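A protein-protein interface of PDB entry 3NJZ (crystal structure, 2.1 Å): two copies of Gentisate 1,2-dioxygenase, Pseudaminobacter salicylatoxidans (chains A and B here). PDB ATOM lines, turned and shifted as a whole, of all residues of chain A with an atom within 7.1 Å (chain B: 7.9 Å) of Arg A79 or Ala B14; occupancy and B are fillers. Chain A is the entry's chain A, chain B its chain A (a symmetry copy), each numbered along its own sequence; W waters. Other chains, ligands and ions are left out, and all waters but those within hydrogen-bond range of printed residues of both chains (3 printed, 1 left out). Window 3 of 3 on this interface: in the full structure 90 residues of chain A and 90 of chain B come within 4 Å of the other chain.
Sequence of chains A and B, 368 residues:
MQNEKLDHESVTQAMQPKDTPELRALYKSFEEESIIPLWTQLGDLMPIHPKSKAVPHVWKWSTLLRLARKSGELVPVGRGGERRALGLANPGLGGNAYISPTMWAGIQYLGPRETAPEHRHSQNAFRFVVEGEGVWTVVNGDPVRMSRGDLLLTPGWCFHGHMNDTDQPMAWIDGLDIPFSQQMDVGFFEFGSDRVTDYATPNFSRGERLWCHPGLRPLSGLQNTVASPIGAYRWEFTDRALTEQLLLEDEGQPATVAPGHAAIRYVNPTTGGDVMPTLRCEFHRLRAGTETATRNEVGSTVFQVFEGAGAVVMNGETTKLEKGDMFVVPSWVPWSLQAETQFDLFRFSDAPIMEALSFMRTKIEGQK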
ATOM      1  N   VAL A  75     -18.860 -26.059  -4.893  1.00  0.00           N
ATOM      2  CA  VAL A  75     -17.735 -25.897  -5.794  1.00  0.00           C
ATOM      3  C   VAL A  75     -17.154 -24.498  -5.681  1.00  0.00           C
ATOM      4  O   VAL A  75     -17.836 -23.525  -5.986  1.00  0.00           O
ATOM      5  CB  VAL A  75     -18.127 -26.192  -7.254  1.00  0.00           C
ATOM      6  CG1 VAL A  75     -16.910 -26.023  -8.202  1.00  0.00           C
ATOM      7  CG2 VAL A  75     -18.723 -27.576  -7.378  1.00  0.00           C
ATOM      8  N   PRO A  76     -15.873 -24.393  -5.271  1.00  0.00           N
ATOM      9  CA  PRO A  76     -15.242 -23.068  -5.275  1.00  0.00           C
ATOM     10  C   PRO A  76     -14.917 -22.623  -6.718  1.00  0.00           C
ATOM     11  O   PRO A  76     -14.654 -23.465  -7.589  1.00  0.00           O
ATOM     12  CB  PRO A  76     -13.964 -23.263  -4.455  1.00  0.00           C
ATOM     13  CG  PRO A  76     -13.648 -24.742  -4.522  1.00  0.00           C
ATOM     14  CD  PRO A  76     -14.894 -25.482  -5.063  1.00  0.00           C
ATOM     15  N   VAL A  77     -14.986 -21.307  -6.952  1.00  0.00           N
ATOM     16  CA  VAL A  77     -14.646 -20.715  -8.241  1.00  0.00           C
ATOM     17  C   VAL A  77     -13.189 -20.230  -8.169  1.00  0.00           C
ATOM     18  O   VAL A  77     -12.698 -19.861  -7.096  1.00  0.00           O
ATOM     19  CB  VAL A  77     -15.615 -19.552  -8.608  1.00  0.00           C
ATOM     20  CG1 VAL A  77     -15.467 -18.395  -7.620  1.00  0.00           C
ATOM     21  CG2 VAL A  77     -15.401 -19.083 -10.021  1.00  0.00           C
ATOM     22  N   GLY A  78     -12.497 -20.248  -9.305  1.00  0.00           N
ATOM     23  CA  GLY A  78     -11.119 -19.785  -9.341  1.00  0.00           C
ATOM     24  C   GLY A  78     -10.382 -20.309 -10.546  1.00  0.00           C
ATOM     25  O   GLY A  78     -11.006 -20.830 -11.494  1.00  0.00           O
ATOM     26  N   ARG A  79      -9.071 -20.178 -10.529  1.00  0.00           N
ATOM     27  CA  ARG A  79      -8.200 -20.605 -11.591  1.00  0.00           C
ATOM     28  C   ARG A  79      -8.337 -22.044 -12.053  1.00  0.00           C
ATOM     29  O   ARG A  79      -8.572 -22.916 -11.278  1.00  0.00           O
ATOM     30  CB  ARG A  79      -6.756 -20.352 -11.184  1.00  0.00           C
ATOM     31  CG  ARG A  79      -5.856 -19.996 -12.311  1.00  0.00           C
ATOM     32  CD  ARG A  79      -6.556 -19.133 -13.316  1.00  0.00           C
ATOM     33  NE  ARG A  79      -5.980 -17.837 -13.307  1.00  0.00           N
ATOM     34  CZ  ARG A  79      -6.291 -16.848 -14.108  1.00  0.00           C
ATOM     35  NH1 ARG A  79      -7.220 -16.978 -15.014  1.00  0.00           N
ATOM     36  NH2 ARG A  79      -5.625 -15.730 -13.985  1.00  0.00           N
ATOM     37  N   GLY A  80      -8.147 -22.282 -13.327  1.00  0.00           N
ATOM     38  CA  GLY A  80      -8.143 -23.656 -13.862  1.00  0.00           C
ATOM     39  C   GLY A  80      -9.480 -23.975 -14.511  1.00  0.00           C
ATOM     40  O   GLY A  80      -9.589 -23.995 -15.757  1.00  0.00           O
ATOM     41  N   GLY A  81     -10.478 -24.198 -13.643  1.00  0.00           N
ATOM     42  CA  GLY A  81     -11.890 -24.274 -14.002  1.00  0.00           C
ATOM     43  C   GLY A  81     -12.452 -22.911 -14.419  1.00  0.00           C
ATOM     44  O   GLY A  81     -13.409 -22.861 -15.177  1.00  0.00           O
ATOM     45  N   GLU A  82     -11.874 -21.815 -13.909  1.00  0.00           N
ATOM     46  CA  GLU A  82     -12.197 -20.416 -14.340  1.00  0.00           C
ATOM     47  C   GLU A  82     -13.564 -19.823 -13.944  1.00  0.00           C
ATOM     48  O   GLU A  82     -13.642 -18.681 -13.439  1.00  0.00           O
ATOM     49  CB  GLU A  82     -11.992 -20.233 -15.855  1.00  0.00           C
ATOM     50  CG  GLU A  82     -10.551 -20.437 -16.330  1.00  0.00           C
ATOM     51  CD  GLU A  82      -9.568 -19.484 -15.647  1.00  0.00           C
ATOM     52  OE1 GLU A  82      -9.683 -18.237 -15.852  1.00  0.00           O
ATOM     53  OE2 GLU A  82      -8.681 -20.001 -14.907  1.00  0.00           O
ATOM     54  N   ARG A  83     -14.637 -20.580 -14.193  1.00  0.00           N
ATOM     55  CA  ARG A  83     -15.999 -20.077 -14.028  1.00  0.00           C
ATOM     56  C   ARG A  83     -16.871 -21.173 -13.424  1.00  0.00           C
ATOM     57  O   ARG A  83     -16.744 -22.320 -13.787  1.00  0.00           O
ATOM     58  CB  ARG A  83     -16.573 -19.638 -15.397  1.00  0.00           C
ATOM     59  CG  ARG A  83     -15.694 -18.624 -16.186  1.00  0.00           C
ATOM     60  CD  ARG A  83     -15.658 -17.270 -15.488  1.00  0.00           C
ATOM     61  NE  ARG A  83     -14.954 -16.229 -16.239  1.00  0.00           N
ATOM     62  CZ  ARG A  83     -13.701 -15.822 -15.995  1.00  0.00           C
ATOM     63  NH1 ARG A  83     -12.984 -16.393 -15.017  1.00  0.00           N
ATOM     64  NH2 ARG A  83     -13.166 -14.822 -16.711  1.00  0.00           N
ATOM     65  N   THR A 115     -14.438 -13.506  -6.637  1.00  0.00           N
ATOM     66  CA  THR A 115     -13.807 -13.058  -7.860  1.00  0.00           C
ATOM     67  C   THR A 115     -13.671 -14.266  -8.811  1.00  0.00           C
ATOM     68  O   THR A 115     -13.352 -15.385  -8.375  1.00  0.00           O
ATOM     69  CB  THR A 115     -12.423 -12.445  -7.538  1.00  0.00           C
ATOM     70  OG1 THR A 115     -12.617 -11.137  -7.007  1.00  0.00           O
ATOM     71  CG2 THR A 115     -11.502 -12.362  -8.786  1.00  0.00           C
ATOM     72  N   ALA A 116     -13.967 -14.048 -10.091  1.00  0.00           N
ATOM     73  CA  ALA A 116     -13.612 -15.011 -11.156  1.00  0.00           C
ATOM     74  C   ALA A 116     -12.456 -14.415 -11.982  1.00  0.00           C
ATOM     75  O   ALA A 116     -12.602 -13.337 -12.527  1.00  0.00           O
ATOM     76  CB  ALA A 116     -14.837 -15.339 -12.027  1.00  0.00           C
ATOM     77  N   PRO A 117     -11.291 -15.102 -12.044  1.00  0.00           N
ATOM     78  CA  PRO A 117     -10.070 -14.424 -12.504  1.00  0.00           C
ATOM     79  C   PRO A 117     -10.019 -14.124 -14.019  1.00  0.00           C
ATOM     80  O   PRO A 117     -10.778 -14.694 -14.802  1.00  0.00           O
ATOM     81  CB  PRO A 117      -8.952 -15.397 -12.099  1.00  0.00           C
ATOM     82  CG  PRO A 117      -9.603 -16.729 -12.110  1.00  0.00           C
ATOM     83  CD  PRO A 117     -11.046 -16.521 -11.720  1.00  0.00           C
ATOM     84  N   GLU A 118      -9.094 -13.247 -14.396  1.00  0.00           N
ATOM     85  CA  GLU A 118      -9.056 -12.678 -15.716  1.00  0.00           C
ATOM     86  C   GLU A 118      -8.468 -13.621 -16.746  1.00  0.00           C
ATOM     87  O   GLU A 118      -7.462 -14.323 -16.478  1.00  0.00           O
ATOM     88  CB  GLU A 118      -8.274 -11.374 -15.721  1.00  0.00           C
ATOM     89  CG  GLU A 118      -9.086 -10.206 -15.123  1.00  0.00           C
ATOM     90  CD  GLU A 118      -8.629  -8.842 -15.620  1.00  0.00           C
ATOM     91  OE1 GLU A 118      -7.703  -8.781 -16.479  1.00  0.00           O
ATOM     92  OE2 GLU A 118      -9.197  -7.836 -15.129  1.00  0.00           O
ATOM     93  N   HIS A 119      -9.076 -13.610 -17.929  1.00  0.00           N
ATOM     94  CA  HIS A 119      -8.536 -14.354 -19.050  1.00  0.00           C
ATOM     95  C   HIS A 119      -9.048 -13.810 -20.389  1.00  0.00           C
ATOM     96  O   HIS A 119      -9.902 -12.931 -20.404  1.00  0.00           O
ATOM     97  CB  HIS A 119      -8.794 -15.865 -18.885  1.00  0.00           C
ATOM     98  CG  HIS A 119     -10.245 -16.255 -18.871  1.00  0.00           C
ATOM     99  ND1 HIS A 119     -11.172 -15.750 -19.761  1.00  0.00           N
ATOM    100  CD2 HIS A 119     -10.908 -17.153 -18.110  1.00  0.00           C
ATOM    101  CE1 HIS A 119     -12.347 -16.307 -19.528  1.00  0.00           C
ATOM    102  NE2 HIS A 119     -12.210 -17.175 -18.541  1.00  0.00           N
ATOM    103  N   HIS A 160     -11.198 -10.461 -19.648  1.00  0.00           N
ATOM    104  CA  HIS A 160     -12.366 -10.272 -18.776  1.00  0.00           C
ATOM    105  C   HIS A 160     -12.247 -11.100 -17.483  1.00  0.00           C
ATOM    106  O   HIS A 160     -11.727 -12.225 -17.496  1.00  0.00           O
ATOM    107  CB  HIS A 160     -13.689 -10.587 -19.496  1.00  0.00           C
ATOM    108  CG  HIS A 160     -13.748 -11.962 -20.086  1.00  0.00           C
ATOM    109  ND1 HIS A 160     -13.026 -12.313 -21.207  1.00  0.00           N
ATOM    110  CD2 HIS A 160     -14.418 -13.077 -19.703  1.00  0.00           C
ATOM    111  CE1 HIS A 160     -13.260 -13.582 -21.495  1.00  0.00           C
ATOM    112  NE2 HIS A 160     -14.105 -14.067 -20.603  1.00  0.00           N
ATOM    113  N   PHE A 189      -6.478 -19.256 -26.198  1.00  0.00           N
ATOM    114  CA  PHE A 189      -6.817 -18.914 -24.813  1.00  0.00           C
ATOM    115  C   PHE A 189      -5.582 -18.408 -24.108  1.00  0.00           C
ATOM    116  O   PHE A 189      -4.477 -18.937 -24.326  1.00  0.00           O
ATOM    117  CB  PHE A 189      -7.322 -20.149 -24.073  1.00  0.00           C
ATOM    118  CG  PHE A 189      -7.830 -19.869 -22.681  1.00  0.00           C
ATOM    119  CD1 PHE A 189      -6.933 -19.777 -21.595  1.00  0.00           C
ATOM    120  CD2 PHE A 189      -9.199 -19.736 -22.437  1.00  0.00           C
ATOM    121  CE1 PHE A 189      -7.400 -19.530 -20.287  1.00  0.00           C
ATOM    122  CE2 PHE A 189      -9.675 -19.492 -21.125  1.00  0.00           C
ATOM    123  CZ  PHE A 189      -8.779 -19.382 -20.061  1.00  0.00           C
ATOM    124  N   GLU A 190      -5.771 -17.388 -23.267  1.00  0.00           N
ATOM    125  CA  GLU A 190      -4.678 -16.866 -22.472  1.00  0.00           C
ATOM    126  C   GLU A 190      -5.138 -16.537 -21.045  1.00  0.00           C
ATOM    127  O   GLU A 190      -6.162 -15.859 -20.855  1.00  0.00           O
ATOM    128  CB  GLU A 190      -4.080 -15.653 -23.165  1.00  0.00           C
ATOM    129  CG  GLU A 190      -2.865 -15.109 -22.499  1.00  0.00           C
ATOM    130  CD  GLU A 190      -2.355 -13.855 -23.178  1.00  0.00           C
ATOM    131  OE1 GLU A 190      -1.626 -13.093 -22.495  1.00  0.00           O
ATOM    132  OE2 GLU A 190      -2.683 -13.626 -24.374  1.00  0.00           O
ATOM    133  N   PHE A 191      -4.401 -17.039 -20.046  1.00  0.00           N
ATOM    134  CA  PHE A 191      -4.682 -16.699 -18.636  1.00  0.00           C
ATOM    135  C   PHE A 191      -4.231 -15.258 -18.343  1.00  0.00           C
ATOM    136  O   PHE A 191      -3.140 -14.857 -18.749  1.00  0.00           O
ATOM    137  CB  PHE A 191      -3.996 -17.679 -17.663  1.00  0.00           C
ATOM    138  CG  PHE A 191      -4.557 -19.071 -17.705  1.00  0.00           C
ATOM    139  CD1 PHE A 191      -5.729 -19.380 -17.024  1.00  0.00           C
ATOM    140  CD2 PHE A 191      -3.914 -20.073 -18.433  1.00  0.00           C
ATOM    141  CE1 PHE A 191      -6.253 -20.674 -17.062  1.00  0.00           C
ATOM    142  CE2 PHE A 191      -4.425 -21.370 -18.490  1.00  0.00           C
ATOM    143  CZ  PHE A 191      -5.604 -21.675 -17.802  1.00  0.00           C
ATOM    144  N   GLY A 192      -5.075 -14.489 -17.654  1.00  0.00           N
ATOM    145  CA  GLY A 192      -4.727 -13.120 -17.224  1.00  0.00           C
ATOM    146  C   GLY A 192      -4.427 -13.056 -15.730  1.00  0.00           C
ATOM    147  O   GLY A 192      -4.015 -14.045 -15.132  1.00  0.00           O
ATOM    148  N   SER A 193      -4.633 -11.905 -15.103  1.00  0.00           N
ATOM    149  CA  SER A 193      -4.404 -11.840 -13.654  1.00  0.00           C
ATOM    150  C   SER A 193      -5.418 -12.688 -12.841  1.00  0.00           C
ATOM    151  O   SER A 193      -6.590 -12.835 -13.227  1.00  0.00           O
ATOM    152  CB  SER A 193      -4.349 -10.396 -13.153  1.00  0.00           C
ATOM    153  OG  SER A 193      -5.648  -9.899 -12.919  1.00  0.00           O
ATOM    154  N   ASP A 194      -4.930 -13.233 -11.723  1.00  0.00           N
ATOM    155  CA  ASP A 194      -5.705 -14.052 -10.785  1.00  0.00           C
ATOM    156  C   ASP A 194      -6.846 -13.326 -10.082  1.00  0.00           C
ATOM    157  O   ASP A 194      -7.757 -13.965  -9.566  1.00  0.00           O
ATOM    158  CB  ASP A 194      -4.774 -14.663  -9.718  1.00  0.00           C
ATOM    159  CG  ASP A 194      -3.889 -15.777 -10.268  1.00  0.00           C
ATOM    160  OD1 ASP A 194      -4.037 -16.151 -11.460  1.00  0.00           O
ATOM    161  OD2 ASP A 194      -3.034 -16.280  -9.498  1.00  0.00           O
ATOM    162  N   ARG A 195      -6.766 -12.003 -10.006  1.00  0.00           N
ATOM    163  CA  ARG A 195      -7.856 -11.172  -9.485  1.00  0.00           C
ATOM    164  C   ARG A 195      -8.317 -10.319 -10.678  1.00  0.00           C
ATOM    165  O   ARG A 195      -7.804 -10.505 -11.778  1.00  0.00           O
ATOM    166  CB  ARG A 195      -7.357 -10.307  -8.315  1.00  0.00           C
ATOM    167  CG  ARG A 195      -7.055 -11.104  -7.010  1.00  0.00           C
ATOM    168  N   GLU B   4       0.401 -15.576 -18.652  1.00  0.00           N
ATOM    169  CA  GLU B   4       0.673 -15.516 -20.118  1.00  0.00           C
ATOM    170  C   GLU B   4       1.334 -16.811 -20.635  1.00  0.00           C
ATOM    171  O   GLU B   4       0.897 -17.368 -21.648  1.00  0.00           O
ATOM    172  CB  GLU B   4       1.518 -14.280 -20.471  1.00  0.00           C
ATOM    173  N   LEU B   6       1.463 -19.629 -18.848  1.00  0.00           N
ATOM    174  CA  LEU B   6       0.678 -20.755 -18.312  1.00  0.00           C
ATOM    175  C   LEU B   6      -0.163 -21.432 -19.387  1.00  0.00           C
ATOM    176  O   LEU B   6      -0.703 -20.760 -20.287  1.00  0.00           O
ATOM    177  CB  LEU B   6      -0.292 -20.289 -17.231  1.00  0.00           C
ATOM    178  CG  LEU B   6       0.188 -19.791 -15.886  1.00  0.00           C
ATOM    179  CD1 LEU B   6      -0.960 -19.028 -15.229  1.00  0.00           C
ATOM    180  CD2 LEU B   6       0.672 -20.956 -15.025  1.00  0.00           C
ATOM    181  N   VAL B  11      -1.357 -24.736 -15.149  1.00  0.00           N
ATOM    182  CA  VAL B  11      -2.174 -23.827 -14.317  1.00  0.00           C
ATOM    183  C   VAL B  11      -2.668 -24.545 -13.055  1.00  0.00           C
ATOM    184  O   VAL B  11      -2.979 -25.741 -13.100  1.00  0.00           O
ATOM    185  CB  VAL B  11      -3.391 -23.244 -15.112  1.00  0.00           C
ATOM    186  CG1 VAL B  11      -4.453 -24.314 -15.392  1.00  0.00           C
ATOM    187  CG2 VAL B  11      -3.995 -22.060 -14.401  1.00  0.00           C
ATOM    188  N   THR B  12      -2.719 -23.821 -11.935  1.00  0.00           N
ATOM    189  CA  THR B  12      -3.371 -24.313 -10.716  1.00  0.00           C
ATOM    190  C   THR B  12      -4.848 -24.610 -10.994  1.00  0.00           C
ATOM    191  O   THR B  12      -5.577 -23.754 -11.537  1.00  0.00           O
ATOM    192  CB  THR B  12      -3.294 -23.266  -9.553  1.00  0.00           C
ATOM    193  OG1 THR B  12      -1.965 -22.738  -9.453  1.00  0.00           O
ATOM    194  CG2 THR B  12      -3.685 -23.902  -8.209  1.00  0.00           C
ATOM    195  N   GLN B  13      -5.277 -25.822 -10.641  1.00  0.00           N
ATOM    196  CA  GLN B  13      -6.690 -26.206 -10.683  1.00  0.00           C
ATOM    197  C   GLN B  13      -7.381 -25.907  -9.335  1.00  0.00           C
ATOM    198  O   GLN B  13      -7.348 -26.732  -8.421  1.00  0.00           O
ATOM    199  CB  GLN B  13      -6.840 -27.689 -11.064  1.00  0.00           C
ATOM    200  CG  GLN B  13      -6.443 -28.042 -12.512  1.00  0.00           C
ATOM    201  CD  GLN B  13      -7.225 -27.244 -13.575  1.00  0.00           C
ATOM    202  OE1 GLN B  13      -8.390 -26.874 -13.378  1.00  0.00           O
ATOM    203  NE2 GLN B  13      -6.569 -26.969 -14.702  1.00  0.00           N
ATOM    204  N   ALA B  14      -8.001 -24.730  -9.226  1.00  0.00           N
ATOM    205  CA  ALA B  14      -8.616 -24.251  -7.979  1.00  0.00           C
ATOM    206  C   ALA B  14     -10.132 -24.536  -7.816  1.00  0.00           C
ATOM    207  O   ALA B  14     -10.739 -24.109  -6.827  1.00  0.00           O
ATOM    208  CB  ALA B  14      -8.325 -22.740  -7.788  1.00  0.00           C
ATOM    209  N   MET B  15     -10.734 -25.260  -8.761  1.00  0.00           N
ATOM    210  CA  MET B  15     -12.165 -25.623  -8.676  1.00  0.00           C
ATOM    211  C   MET B  15     -12.380 -27.129  -8.502  1.00  0.00           C
ATOM    212  O   MET B  15     -13.236 -27.727  -9.168  1.00  0.00           O
ATOM    213  CB  MET B  15     -12.936 -25.111  -9.905  1.00  0.00           C
ATOM    214  CG  MET B  15     -12.879 -23.593 -10.029  1.00  0.00           C
ATOM    215  SD  MET B  15     -13.946 -22.814 -11.261  1.00  0.00           S
ATOM    216  CE  MET B  15     -15.606 -23.347 -10.752  1.00  0.00           C
ATOM    217  N   GLN B  16     -11.589 -27.744  -7.631  1.00  0.00           N
ATOM    218  CA  GLN B  16     -11.730 -29.173  -7.360  1.00  0.00           C
ATOM    219  C   GLN B  16     -12.598 -29.297  -6.127  1.00  0.00           C
ATOM    220  O   GLN B  16     -12.157 -29.008  -5.031  1.00  0.00           O
ATOM    221  CB  GLN B  16     -10.368 -29.831  -7.143  1.00  0.00           C
ATOM    222  CG  GLN B  16      -9.249 -29.126  -7.907  1.00  0.00           C
ATOM    223  CD  GLN B  16      -8.081 -30.032  -8.260  1.00  0.00           C
ATOM    224  OE1 GLN B  16      -6.932 -29.759  -7.888  1.00  0.00           O
ATOM    225  NE2 GLN B  16      -8.362 -31.102  -8.999  1.00  0.00           N
ATOM    226  N   PRO B  17     -13.862 -29.681  -6.304  1.00  0.00           N
ATOM    227  CA  PRO B  17     -14.716 -29.768  -5.118  1.00  0.00           C
ATOM    228  C   PRO B  17     -14.365 -30.993  -4.251  1.00  0.00           C
ATOM    229  O   PRO B  17     -13.776 -31.954  -4.742  1.00  0.00           O
ATOM    230  CB  PRO B  17     -16.115 -29.915  -5.707  1.00  0.00           C
ATOM    231  CG  PRO B  17     -15.887 -30.558  -7.045  1.00  0.00           C
ATOM    232  CD  PRO B  17     -14.510 -30.186  -7.520  1.00  0.00           C
ATOM    233  N   TRP B  39     -16.272 -26.216 -15.438  1.00  0.00           N
ATOM    234  CA  TRP B  39     -15.061 -26.376 -14.661  1.00  0.00           C
ATOM    235  C   TRP B  39     -14.408 -27.741 -14.808  1.00  0.00           C
ATOM    236  O   TRP B  39     -13.206 -27.845 -14.604  1.00  0.00           O
ATOM    237  CB  TRP B  39     -15.272 -26.004 -13.181  1.00  0.00           C
ATOM    238  CG  TRP B  39     -16.297 -26.814 -12.427  1.00  0.00           C
ATOM    239  CD1 TRP B  39     -16.081 -27.986 -11.758  1.00  0.00           C
ATOM    240  CD2 TRP B  39     -17.682 -26.488 -12.229  1.00  0.00           C
ATOM    241  NE1 TRP B  39     -17.253 -28.419 -11.168  1.00  0.00           N
ATOM    242  CE2 TRP B  39     -18.244 -27.513 -11.435  1.00  0.00           C
ATOM    243  CE3 TRP B  39     -18.499 -25.429 -12.645  1.00  0.00           C
ATOM    244  CZ2 TRP B  39     -19.594 -27.513 -11.049  1.00  0.00           C
ATOM    245  CZ3 TRP B  39     -19.834 -25.433 -12.271  1.00  0.00           C
ATOM    246  CH2 TRP B  39     -20.374 -26.473 -11.488  1.00  0.00           C
ATOM    247  N   LEU B  42     -12.931 -27.178 -19.062  1.00  0.00           N
ATOM    248  CA  LEU B  42     -12.434 -25.909 -19.633  1.00  0.00           C
ATOM    249  C   LEU B  42     -11.338 -26.045 -20.696  1.00  0.00           C
ATOM    250  O   LEU B  42     -11.441 -25.439 -21.772  1.00  0.00           O
ATOM    251  CB  LEU B  42     -12.032 -24.890 -18.532  1.00  0.00           C
ATOM    252  CG  LEU B  42     -11.794 -23.469 -19.089  1.00  0.00           C
ATOM    253  CD1 LEU B  42     -12.705 -22.426 -18.483  1.00  0.00           C
ATOM    254  CD2 LEU B  42     -10.365 -23.026 -19.012  1.00  0.00           C
HETATM  255  O   HOH W   1      -7.654 -24.893 -17.193  1.00  0.00           O
HETATM  256  O   HOH W   2     -10.675 -22.018  -5.334  1.00  0.00           O
HETATM  257  O   HOH W   3      -1.778 -18.029 -20.547  1.00  0.00           O
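O of Thr B12 sits close to O of Arg A79 (3.1 Å).
The backbone carbonyl oxygen (O) of Arg A79 lies within hydrogen-bond range of the backbone NH (N) of Ala B14, 2.8 Å away.
The side-chain sulfur (SD) of Met B15 lies within hydrogen-bond range of the backbone NH (N) of Glu A82 (3.5 Å).
The backbone NH (N) of Arg A83 is in hydrogen-bond range of the side-chain sulfur (SD) of Met B15, 3.8 Å away.
SD of Met B15 sits close to O of Pro A76 (3.8 Å).
N of Gly A80 sits at hydrogen-bond distance from O of Thr B12 (3.5 Å).
N of Gly A81 lies within hydrogen-bond range of OE1 of Gln B13 (3.4 Å).
N of Gly A78 lies close to SD of Met B15, at 3.5 Å.
Of the printed residues of chain B, Pro A76 touches Ala B14 (3.8 Å) and Met B15 (3.0 Å).
Gly A78 touches one residue of chain B.
Arg A79 touches just these residues of chain B: Val B11 (3.5 Å), Thr B12 (3.1 Å), Gln B13 (3.8 Å) and Ala B14 (2.8 Å).
Printed residues of chain B within 4 Å of Glu A82: Met B15 (3.5 Å) and Leu B42 (3.5 Å).
Printed residues of chain B within 4 Å of Arg A83: Met B15 and Trp B39.
Printed residues of chain B within 4 Å of Phe A191: Glu B4, Leu B6 and Val B11.
Printed residues of chain A within 4 Å of Met B15: Val A75 (3.9 Å), Pro A76 (3.0 Å), Val A77 (3.7 Å), Gly A78 (3.4 Å), Gly A81 (3.5 Å), Glu A82 (3.5 Å) and Arg A83 (3.4 Å).
The nearest residue of chain A that does not touch Ala B14 is Gly A78 (4.2 Å).
Of the 22 printed residues of chain A, 11 touch a printed residue of chain B.
Of the 11 printed residues of chain B, 10 touch a printed residue of chain A.
No position is printed for both chains.
Of the 26 pairs that touch across the chains among the printed residues, none has its exchanged pair printed and touching as well.
Met B15 touches Val A75.
CG2 of Val A75 touches CB of Pro B17, 3.9 Å away.
Val A75 touches Trp B39.
Ala B14 touches Pro A76 (O to CG, 3.8 Å).
O of Gly A80 touches CD2 of Leu B42 (3.5 Å).
C of Gly A81 touches SD of Met B15, 3.5 Å away.
CD1 of Leu B42 touches O of Gly A81, 3.4 Å away.
CD1 of Leu B42 touches CB of Glu A82, 3.5 Å away.
Glu B4 touches Phe A191 (N to O, 3.6 Å).
CD2 of Phe A191 touches O of Leu B6, at 3.8 Å.
Water W2 bridges O of Ala B14 (2.6 Å) and O of Val A77 (3.4 Å).
Water W1 lies within hydrogen-bond range of the backbone carbonyl oxygen of Gly A80 and the side-chain amide nitrogen of Gln B13.
Water W3 lies within hydrogen-bond range of the backbone NH of Phe A191, the backbone carbonyl oxygen of Leu B6 and the backbone carbonyl oxygen of Glu B4.
The guanidinium group (NH2) of Arg A79 is in salt-bridge range of the side-chain carboxylate (OD1) of Asp A194 (3.0 Å).
NH2 of Arg A79 is in hydrogen-bond range of O of Gly A192, 2.6 Å away.
OE1 of Glu A82 is in salt-bridge range of NH1 of Arg A83 (3.9 Å).
N of Gly A80 is in hydrogen-bond range of OE2 of Glu A82 (2.8 Å).
The side-chain amide oxygen (OE1) of Gln B16 lies close to the backbone carbonyl oxygen (O) of Gln B13, 3.1 Å away.
OE1 of Glu A82 is in salt-bridge range of NH1 of Arg A79.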
